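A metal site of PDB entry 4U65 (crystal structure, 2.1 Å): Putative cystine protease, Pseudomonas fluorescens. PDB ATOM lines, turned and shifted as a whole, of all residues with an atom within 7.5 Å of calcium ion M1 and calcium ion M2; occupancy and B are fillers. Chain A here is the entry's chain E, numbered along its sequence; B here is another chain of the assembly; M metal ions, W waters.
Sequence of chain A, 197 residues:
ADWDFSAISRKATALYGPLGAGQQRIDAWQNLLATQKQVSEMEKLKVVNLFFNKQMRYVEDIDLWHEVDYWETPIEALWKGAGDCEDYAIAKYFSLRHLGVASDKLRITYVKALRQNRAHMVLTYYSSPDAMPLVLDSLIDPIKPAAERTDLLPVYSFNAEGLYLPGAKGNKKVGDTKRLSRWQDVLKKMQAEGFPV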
ATOM      1  N   TYR A  58      15.658   6.208 -12.521  1.00  0.00           N
ATOM      2  CA  TYR A  58      14.694   6.700 -13.504  1.00  0.00           C
ATOM      3  C   TYR A  58      14.384   8.163 -13.203  1.00  0.00           C
ATOM      4  O   TYR A  58      13.808   8.482 -12.163  1.00  0.00           O
ATOM      5  CB  TYR A  58      13.418   5.858 -13.493  1.00  0.00           C
ATOM      6  CG  TYR A  58      12.584   6.043 -14.738  1.00  0.00           C
ATOM      7  CD1 TYR A  58      11.830   7.196 -14.942  1.00  0.00           C
ATOM      8  CD2 TYR A  58      12.548   5.052 -15.720  1.00  0.00           C
ATOM      9  CE1 TYR A  58      11.069   7.358 -16.093  1.00  0.00           C
ATOM     10  CE2 TYR A  58      11.785   5.208 -16.862  1.00  0.00           C
ATOM     11  CZ  TYR A  58      11.053   6.366 -17.043  1.00  0.00           C
ATOM     12  OH  TYR A  58      10.288   6.531 -18.180  1.00  0.00           O
ATOM     13  N   VAL A  59      14.773   9.054 -14.117  1.00  0.00           N
ATOM     14  CA  VAL A  59      14.430  10.468 -14.028  1.00  0.00           C
ATOM     15  C   VAL A  59      14.057  10.969 -15.412  1.00  0.00           C
ATOM     16  O   VAL A  59      14.649  10.558 -16.413  1.00  0.00           O
ATOM     17  CB  VAL A  59      15.567  11.310 -13.393  1.00  0.00           C
ATOM     18  CG1 VAL A  59      16.767  10.440 -13.048  1.00  0.00           C
ATOM     19  CG2 VAL A  59      15.973  12.473 -14.280  1.00  0.00           C
ATOM     20  N   GLU A  60      13.041  11.820 -15.471  1.00  0.00           N
ATOM     21  CA  GLU A  60      12.522  12.316 -16.749  1.00  0.00           C
ATOM     22  C   GLU A  60      13.564  13.183 -17.453  1.00  0.00           C
ATOM     23  O   GLU A  60      14.425  13.802 -16.824  1.00  0.00           O
ATOM     24  CB  GLU A  60      11.240  13.116 -16.519  1.00  0.00           C
ATOM     25  CG  GLU A  60      10.152  12.386 -15.728  1.00  0.00           C
ATOM     26  CD  GLU A  60       9.601  11.173 -16.455  1.00  0.00           C
ATOM     27  OE1 GLU A  60       9.691  11.127 -17.701  1.00  0.00           O
ATOM     28  OE2 GLU A  60       9.068  10.261 -15.780  1.00  0.00           O
ATOM     29  N   ASP A  61      13.463  13.225 -18.783  1.00  0.00           N
ATOM     30  CA  ASP A  61      14.445  13.959 -19.578  1.00  0.00           C
ATOM     31  C   ASP A  61      14.419  15.452 -19.270  1.00  0.00           C
ATOM     32  O   ASP A  61      15.457  16.107 -19.287  1.00  0.00           O
ATOM     33  CB  ASP A  61      14.195  13.734 -21.072  1.00  0.00           C
ATOM     34  CG  ASP A  61      14.656  12.365 -21.539  1.00  0.00           C
ATOM     35  OD1 ASP A  61      15.489  11.744 -20.830  1.00  0.00           O
ATOM     36  OD2 ASP A  61      14.203  11.916 -22.608  1.00  0.00           O
ATOM     37  N   ILE A  62      13.234  15.999 -18.977  1.00  0.00           N
ATOM     38  CA  ILE A  62      13.124  17.431 -18.714  1.00  0.00           C
ATOM     39  C   ILE A  62      13.908  17.824 -17.457  1.00  0.00           C
ATOM     40  O   ILE A  62      14.387  18.954 -17.337  1.00  0.00           O
ATOM     41  CB  ILE A  62      11.640  17.854 -18.618  1.00  0.00           C
ATOM     42  CG1 ILE A  62      11.509  19.378 -18.551  1.00  0.00           C
ATOM     43  CG2 ILE A  62      10.964  17.209 -17.408  1.00  0.00           C
ATOM     44  CD1 ILE A  62      12.009  20.084 -19.795  1.00  0.00           C
ATOM     45  N   LEU A  64      16.666  15.837 -16.148  1.00  0.00           N
ATOM     46  CA  LEU A  64      18.078  15.480 -16.269  1.00  0.00           C
ATOM     47  C   LEU A  64      18.771  16.258 -17.389  1.00  0.00           C
ATOM     48  O   LEU A  64      19.935  16.659 -17.248  1.00  0.00           O
ATOM     49  CB  LEU A  64      18.221  13.973 -16.513  1.00  0.00           C
ATOM     50  CG  LEU A  64      19.636  13.382 -16.498  1.00  0.00           C
ATOM     51  CD1 LEU A  64      20.371  13.757 -15.218  1.00  0.00           C
ATOM     52  CD2 LEU A  64      19.581  11.877 -16.674  1.00  0.00           C
ATOM     53  N   TRP A  65      18.073  16.488 -18.496  1.00  0.00           N
ATOM     54  CA  TRP A  65      18.661  17.117 -19.668  1.00  0.00           C
ATOM     55  C   TRP A  65      18.050  18.480 -19.993  1.00  0.00           C
ATOM     56  O   TRP A  65      18.512  19.138 -20.927  1.00  0.00           O
ATOM     57  CB  TRP A  65      18.523  16.187 -20.879  1.00  0.00           C
ATOM     58  CG  TRP A  65      19.190  14.870 -20.656  1.00  0.00           C
ATOM     59  CD1 TRP A  65      18.587  13.695 -20.323  1.00  0.00           C
ATOM     60  CD2 TRP A  65      20.593  14.595 -20.719  1.00  0.00           C
ATOM     61  NE1 TRP A  65      19.529  12.702 -20.174  1.00  0.00           N
ATOM     62  CE2 TRP A  65      20.764  13.237 -20.424  1.00  0.00           C
ATOM     63  CE3 TRP A  65      21.720  15.374 -21.002  1.00  0.00           C
ATOM     64  CZ2 TRP A  65      22.019  12.629 -20.407  1.00  0.00           C
ATOM     65  CZ3 TRP A  65      22.966  14.778 -20.992  1.00  0.00           C
ATOM     66  CH2 TRP A  65      23.101  13.414 -20.686  1.00  0.00           C
ATOM     67  N   GLU A  67      15.398  18.969 -21.423  1.00  0.00           N
ATOM     68  CA  GLU A  67      14.801  18.763 -22.741  1.00  0.00           C
ATOM     69  C   GLU A  67      13.670  17.772 -22.591  1.00  0.00           C
ATOM     70  O   GLU A  67      13.790  16.797 -21.837  1.00  0.00           O
ATOM     71  CB  GLU A  67      15.828  18.251 -23.760  1.00  0.00           C
ATOM     72  CG  GLU A  67      16.908  19.259 -24.119  1.00  0.00           C
ATOM     73  CD  GLU A  67      16.375  20.394 -24.958  1.00  0.00           C
ATOM     74  OE1 GLU A  67      15.277  20.228 -25.533  1.00  0.00           O
ATOM     75  OE2 GLU A  67      17.030  21.448 -25.031  1.00  0.00           O
ATOM     76  N   VAL A  68      12.562  18.018 -23.300  1.00  0.00           N
ATOM     77  CA  VAL A  68      11.400  17.135 -23.182  1.00  0.00           C
ATOM     78  C   VAL A  68      11.773  15.713 -23.573  1.00  0.00           C
ATOM     79  O   VAL A  68      11.383  14.748 -22.893  1.00  0.00           O
ATOM     80  CB  VAL A  68      10.248  17.674 -24.048  1.00  0.00           C
ATOM     81  CG1 VAL A  68       9.127  16.643 -24.140  1.00  0.00           C
ATOM     82  CG2 VAL A  68       9.729  18.978 -23.468  1.00  0.00           C
ATOM     83  N   ASP A  69      12.538  15.552 -24.645  1.00  0.00           N
ATOM     84  CA  ASP A  69      12.983  14.231 -25.081  1.00  0.00           C
ATOM     85  C   ASP A  69      14.462  14.299 -25.432  1.00  0.00           C
ATOM     86  O   ASP A  69      14.887  15.186 -26.184  1.00  0.00           O
ATOM     87  CB  ASP A  69      12.169  13.752 -26.296  1.00  0.00           C
ATOM     88  CG  ASP A  69      12.136  12.244 -26.416  1.00  0.00           C
ATOM     89  OD1 ASP A  69      12.402  11.566 -25.413  1.00  0.00           O
ATOM     90  OD2 ASP A  69      11.841  11.748 -27.522  1.00  0.00           O
ATOM     91  N   TYR A  70      15.243  13.373 -24.873  1.00  0.00           N
ATOM     92  CA  TYR A  70      16.689  13.347 -25.112  1.00  0.00           C
ATOM     93  C   TYR A  70      17.143  11.894 -25.003  1.00  0.00           C
ATOM     94  O   TYR A  70      17.093  11.310 -23.927  1.00  0.00           O
ATOM     95  CB  TYR A  70      17.441  14.227 -24.120  1.00  0.00           C
ATOM     96  CG  TYR A  70      18.929  14.319 -24.387  1.00  0.00           C
ATOM     97  CD1 TYR A  70      19.812  13.412 -23.822  1.00  0.00           C
ATOM     98  CD2 TYR A  70      19.444  15.317 -25.208  1.00  0.00           C
ATOM     99  CE1 TYR A  70      21.169  13.488 -24.077  1.00  0.00           C
ATOM    100  CE2 TYR A  70      20.798  15.401 -25.458  1.00  0.00           C
ATOM    101  CZ  TYR A  70      21.660  14.487 -24.892  1.00  0.00           C
ATOM    102  OH  TYR A  70      23.005  14.570 -25.145  1.00  0.00           O
ATOM    103  N   TRP A  71      17.592  11.327 -26.125  1.00  0.00           N
ATOM    104  CA  TRP A  71      17.992   9.916 -26.168  1.00  0.00           C
ATOM    105  C   TRP A  71      19.469   9.802 -25.784  1.00  0.00           C
ATOM    106  O   TRP A  71      20.341  10.280 -26.507  1.00  0.00           O
ATOM    107  CB  TRP A  71      17.737   9.324 -27.550  1.00  0.00           C
ATOM    108  CG  TRP A  71      16.274   9.142 -27.866  1.00  0.00           C
ATOM    109  CD1 TRP A  71      15.220   9.790 -27.292  1.00  0.00           C
ATOM    110  CD2 TRP A  71      15.713   8.224 -28.814  1.00  0.00           C
ATOM    111  NE1 TRP A  71      14.040   9.340 -27.832  1.00  0.00           N
ATOM    112  CE2 TRP A  71      14.313   8.382 -28.759  1.00  0.00           C
ATOM    113  CE3 TRP A  71      16.258   7.293 -29.699  1.00  0.00           C
ATOM    114  CZ2 TRP A  71      13.446   7.642 -29.568  1.00  0.00           C
ATOM    115  CZ3 TRP A  71      15.398   6.549 -30.498  1.00  0.00           C
ATOM    116  CH2 TRP A  71      14.013   6.731 -30.433  1.00  0.00           C
ATOM    117  N   GLU A  72      19.734   9.164 -24.650  1.00  0.00           N
ATOM    118  CA  GLU A  72      21.086   8.997 -24.151  1.00  0.00           C
ATOM    119  C   GLU A  72      21.821   7.896 -24.899  1.00  0.00           C
ATOM    120  O   GLU A  72      21.235   6.858 -25.240  1.00  0.00           O
ATOM    121  CB  GLU A  72      21.072   8.644 -22.663  1.00  0.00           C
ATOM    122  CG  GLU A  72      20.555   9.725 -21.748  1.00  0.00           C
ATOM    123  CD  GLU A  72      20.414   9.243 -20.318  1.00  0.00           C
ATOM    124  OE1 GLU A  72      20.404   8.007 -20.116  1.00  0.00           O
ATOM    125  OE2 GLU A  72      20.320  10.088 -19.408  1.00  0.00           O
ATOM    126  N   ALA A  82      21.600   7.769 -14.772  1.00  0.00           N
ATOM    127  CA  ALA A  82      20.189   8.099 -14.761  1.00  0.00           C
ATOM    128  C   ALA A  82      19.693   8.278 -16.188  1.00  0.00           C
ATOM    129  O   ALA A  82      20.462   8.572 -17.102  1.00  0.00           O
ATOM    130  CB  ALA A  82      19.927   9.361 -13.940  1.00  0.00           C
ATOM    131  N   GLY A  83      18.389   8.106 -16.357  1.00  0.00           N
ATOM    132  CA  GLY A  83      17.763   8.235 -17.657  1.00  0.00           C
ATOM    133  C   GLY A  83      16.289   7.874 -17.558  1.00  0.00           C
ATOM    134  O   GLY A  83      15.777   7.597 -16.475  1.00  0.00           O
ATOM    135  N   ASP A  84      15.632   7.878 -18.715  1.00  0.00           N
ATOM    136  CA  ASP A  84      14.231   7.487 -18.744  1.00  0.00           C
ATOM    137  C   ASP A  84      14.018   6.281 -19.656  1.00  0.00           C
ATOM    138  O   ASP A  84      14.967   5.566 -19.965  1.00  0.00           O
ATOM    139  CB  ASP A  84      13.336   8.670 -19.149  1.00  0.00           C
ATOM    140  CG  ASP A  84      13.439   9.028 -20.617  1.00  0.00           C
ATOM    141  OD1 ASP A  84      14.393   8.595 -21.293  1.00  0.00           O
ATOM    142  OD2 ASP A  84      12.545   9.748 -21.106  1.00  0.00           O
ATOM    143  N   CYS A  85      12.775   6.083 -20.120  1.00  0.00           N
ATOM    144  CA  CYS A  85      12.365   4.786 -20.661  1.00  0.00           C
ATOM    145  C   CYS A  85      13.240   4.361 -21.841  1.00  0.00           C
ATOM    146  O   CYS A  85      13.745   3.231 -21.863  1.00  0.00           O
ATOM    147  CB  CYS A  85      10.893   4.831 -21.069  1.00  0.00           C
ATOM    148  SG  CYS A  85      10.451   6.101 -22.267  1.00  0.00           S
ATOM    149  N   GLU A  86      13.431   5.241 -22.823  1.00  0.00           N
ATOM    150  CA  GLU A  86      14.188   4.828 -24.005  1.00  0.00           C
ATOM    151  C   GLU A  86      15.676   4.698 -23.706  1.00  0.00           C
ATOM    152  O   GLU A  86      16.364   3.897 -24.351  1.00  0.00           O
ATOM    153  CB  GLU A  86      13.965   5.793 -25.168  1.00  0.00           C
ATOM    154  CG  GLU A  86      14.750   7.085 -25.103  1.00  0.00           C
ATOM    155  CD  GLU A  86      13.979   8.198 -24.434  1.00  0.00           C
ATOM    156  OE1 GLU A  86      14.565   9.286 -24.248  1.00  0.00           O
ATOM    157  OE2 GLU A  86      12.797   7.978 -24.091  1.00  0.00           O
ATOM    158  N   ASP A  87      16.179   5.460 -22.737  1.00  0.00           N
ATOM    159  CA  ASP A  87      17.599   5.368 -22.379  1.00  0.00           C
ATOM    160  C   ASP A  87      17.940   3.964 -21.899  1.00  0.00           C
ATOM    161  O   ASP A  87      18.954   3.391 -22.301  1.00  0.00           O
ATOM    162  CB  ASP A  87      17.938   6.400 -21.301  1.00  0.00           C
ATOM    163  CG  ASP A  87      17.624   7.813 -21.741  1.00  0.00           C
ATOM    164  OD1 ASP A  87      17.704   8.104 -22.960  1.00  0.00           O
ATOM    165  OD2 ASP A  87      17.298   8.638 -20.865  1.00  0.00           O
ATOM    166  N   TYR A  88      17.098   3.392 -21.032  1.00  0.00           N
ATOM    167  CA  TYR A  88      17.291   2.012 -20.592  1.00  0.00           C
ATOM    168  C   TYR A  88      17.288   1.053 -21.782  1.00  0.00           C
ATOM    169  O   TYR A  88      18.167   0.193 -21.899  1.00  0.00           O
ATOM    170  CB  TYR A  88      16.195   1.601 -19.608  1.00  0.00           C
ATOM    171  CG  TYR A  88      16.276   2.204 -18.220  1.00  0.00           C
ATOM    172  CD1 TYR A  88      15.953   3.537 -17.993  1.00  0.00           C
ATOM    173  CD2 TYR A  88      16.624   1.423 -17.127  1.00  0.00           C
ATOM    174  CE1 TYR A  88      15.999   4.080 -16.725  1.00  0.00           C
ATOM    175  CE2 TYR A  88      16.680   1.953 -15.852  1.00  0.00           C
ATOM    176  CZ  TYR A  88      16.367   3.282 -15.651  1.00  0.00           C
ATOM    177  OH  TYR A  88      16.415   3.831 -14.390  1.00  0.00           O
ATOM    178  N   ILE A  90      17.868   1.613 -25.014  1.00  0.00           N
ATOM    179  CA  ILE A  90      19.031   1.795 -25.890  1.00  0.00           C
ATOM    180  C   ILE A  90      20.273   1.167 -25.265  1.00  0.00           C
ATOM    181  O   ILE A  90      21.045   0.472 -25.934  1.00  0.00           O
ATOM    182  CB  ILE A  90      19.253   3.293 -26.179  1.00  0.00           C
ATOM    183  CG1 ILE A  90      18.127   3.837 -27.059  1.00  0.00           C
ATOM    184  CG2 ILE A  90      20.607   3.522 -26.834  1.00  0.00           C
ATOM    185  CD1 ILE A  90      18.102   5.353 -27.156  1.00  0.00           C
ATOM    186  N   MET A 121       8.509   2.997 -23.429  1.00  0.00           N
ATOM    187  CA  MET A 121       9.298   2.204 -24.343  1.00  0.00           C
ATOM    188  C   MET A 121       9.985   1.068 -23.598  1.00  0.00           C
ATOM    189  O   MET A 121      10.453   1.255 -22.474  1.00  0.00           O
ATOM    190  CB  MET A 121      10.348   3.061 -25.065  1.00  0.00           C
ATOM    191  CG  MET A 121      11.218   2.276 -26.026  1.00  0.00           C
ATOM    192  SD  MET A 121      12.439   3.279 -26.869  1.00  0.00           S
ATOM    193  CE  MET A 121      11.389   4.478 -27.693  1.00  0.00           C
ATOM    194  N   ARG A 182      16.214  10.480 -34.506  1.00  0.00           N
ATOM    195  CA  ARG A 182      16.525  10.205 -33.104  1.00  0.00           C
ATOM    196  C   ARG A 182      17.597   9.126 -32.965  1.00  0.00           C
ATOM    197  O   ARG A 182      18.587   9.303 -32.249  1.00  0.00           O
ATOM    198  CB  ARG A 182      15.261   9.787 -32.355  1.00  0.00           C
ATOM    199  CG  ARG A 182      14.285  10.920 -32.081  1.00  0.00           C
ATOM    200  CD  ARG A 182      14.718  11.767 -30.892  1.00  0.00           C
ATOM    201  NE  ARG A 182      13.776  12.852 -30.640  1.00  0.00           N
ATOM    202  CZ  ARG A 182      13.916  13.775 -29.690  1.00  0.00           C
ATOM    203  NH1 ARG A 182      14.983  13.745 -28.898  1.00  0.00           N
ATOM    204  NH2 ARG A 182      13.007  14.718 -29.546  1.00  0.00           N
ATOM    205  N   LYS B  49       4.790   9.585 -31.792  1.00  0.00           N
ATOM    206  CA  LYS B  49       6.203   9.484 -31.443  1.00  0.00           C
ATOM    207  C   LYS B  49       6.913   8.467 -32.317  1.00  0.00           C
ATOM    208  O   LYS B  49       8.027   8.730 -32.803  1.00  0.00           O
ATOM    209  CB  LYS B  49       6.354   9.120 -29.965  1.00  0.00           C
ATOM    210  CG  LYS B  49       6.749  10.270 -29.063  1.00  0.00           C
ATOM    211  CD  LYS B  49       6.716   9.862 -27.596  1.00  0.00           C
ATOM    212  CE  LYS B  49       7.531   8.595 -27.355  1.00  0.00           C
ATOM    213  NZ  LYS B  49       7.650   8.252 -25.908  1.00  0.00           N
HETATM  214 CA    CA M   1      15.981   9.906 -22.449  1.00  0.00          CA
HETATM  215 CA    CA M   2      12.502  10.337 -23.409  1.00  0.00          CA
HETATM  216  O   HOH W   1      10.213   8.998 -23.345  1.00  0.00           O
HETATM  217  O   HOH W   2      10.774  11.981 -22.786  1.00  0.00           O
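Calcium ion M2 is bound by OD1 of Asp 69 (2.4 Å), OD2 of Asp 84 (2.4 Å), OD2 of Asp 61 (2.5 Å), OE1 of Glu 86 (2.5 Å), water W2 (2.5 Å), OE2 of Glu 86 (2.5 Å) and water W1 (2.7 Å).
Calcium ion M1 is bound by O of Tyr 70 (2.3 Å), OD1 of Asp 84 (2.4 Å), OE1 of Glu 86 (2.4 Å), OD2 of Asp 87 (2.4 Å), OD1 of Asp 61 (2.5 Å), OD1 of Asp 87 (2.5 Å) and OD2 of Asp 61 (2.7 Å).
Along chain A the residues within 4 Å of calcium ion M1 span positions 61 to 87.
Within 4 Å of calcium ion M2: Asp 61, Asp 69, Asp 84 and Glu 86. The nearest printed residue that does not touch calcium ion M2 is Tyr 70 (4.3 Å).
OD2 of Asp 69 is in hydrogen-bond range of NE1 of Trp 71 (3.3 Å). NH2 of Arg 182 is in salt-bridge range of OD2 of Asp 69. The side-chain carboxylate of Glu 86 sits close to the side-chain sulfur of Cys 85 (3.5 Å). The side-chain carboxylate of Asp 87 lies close to the backbone NH of Glu 72.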
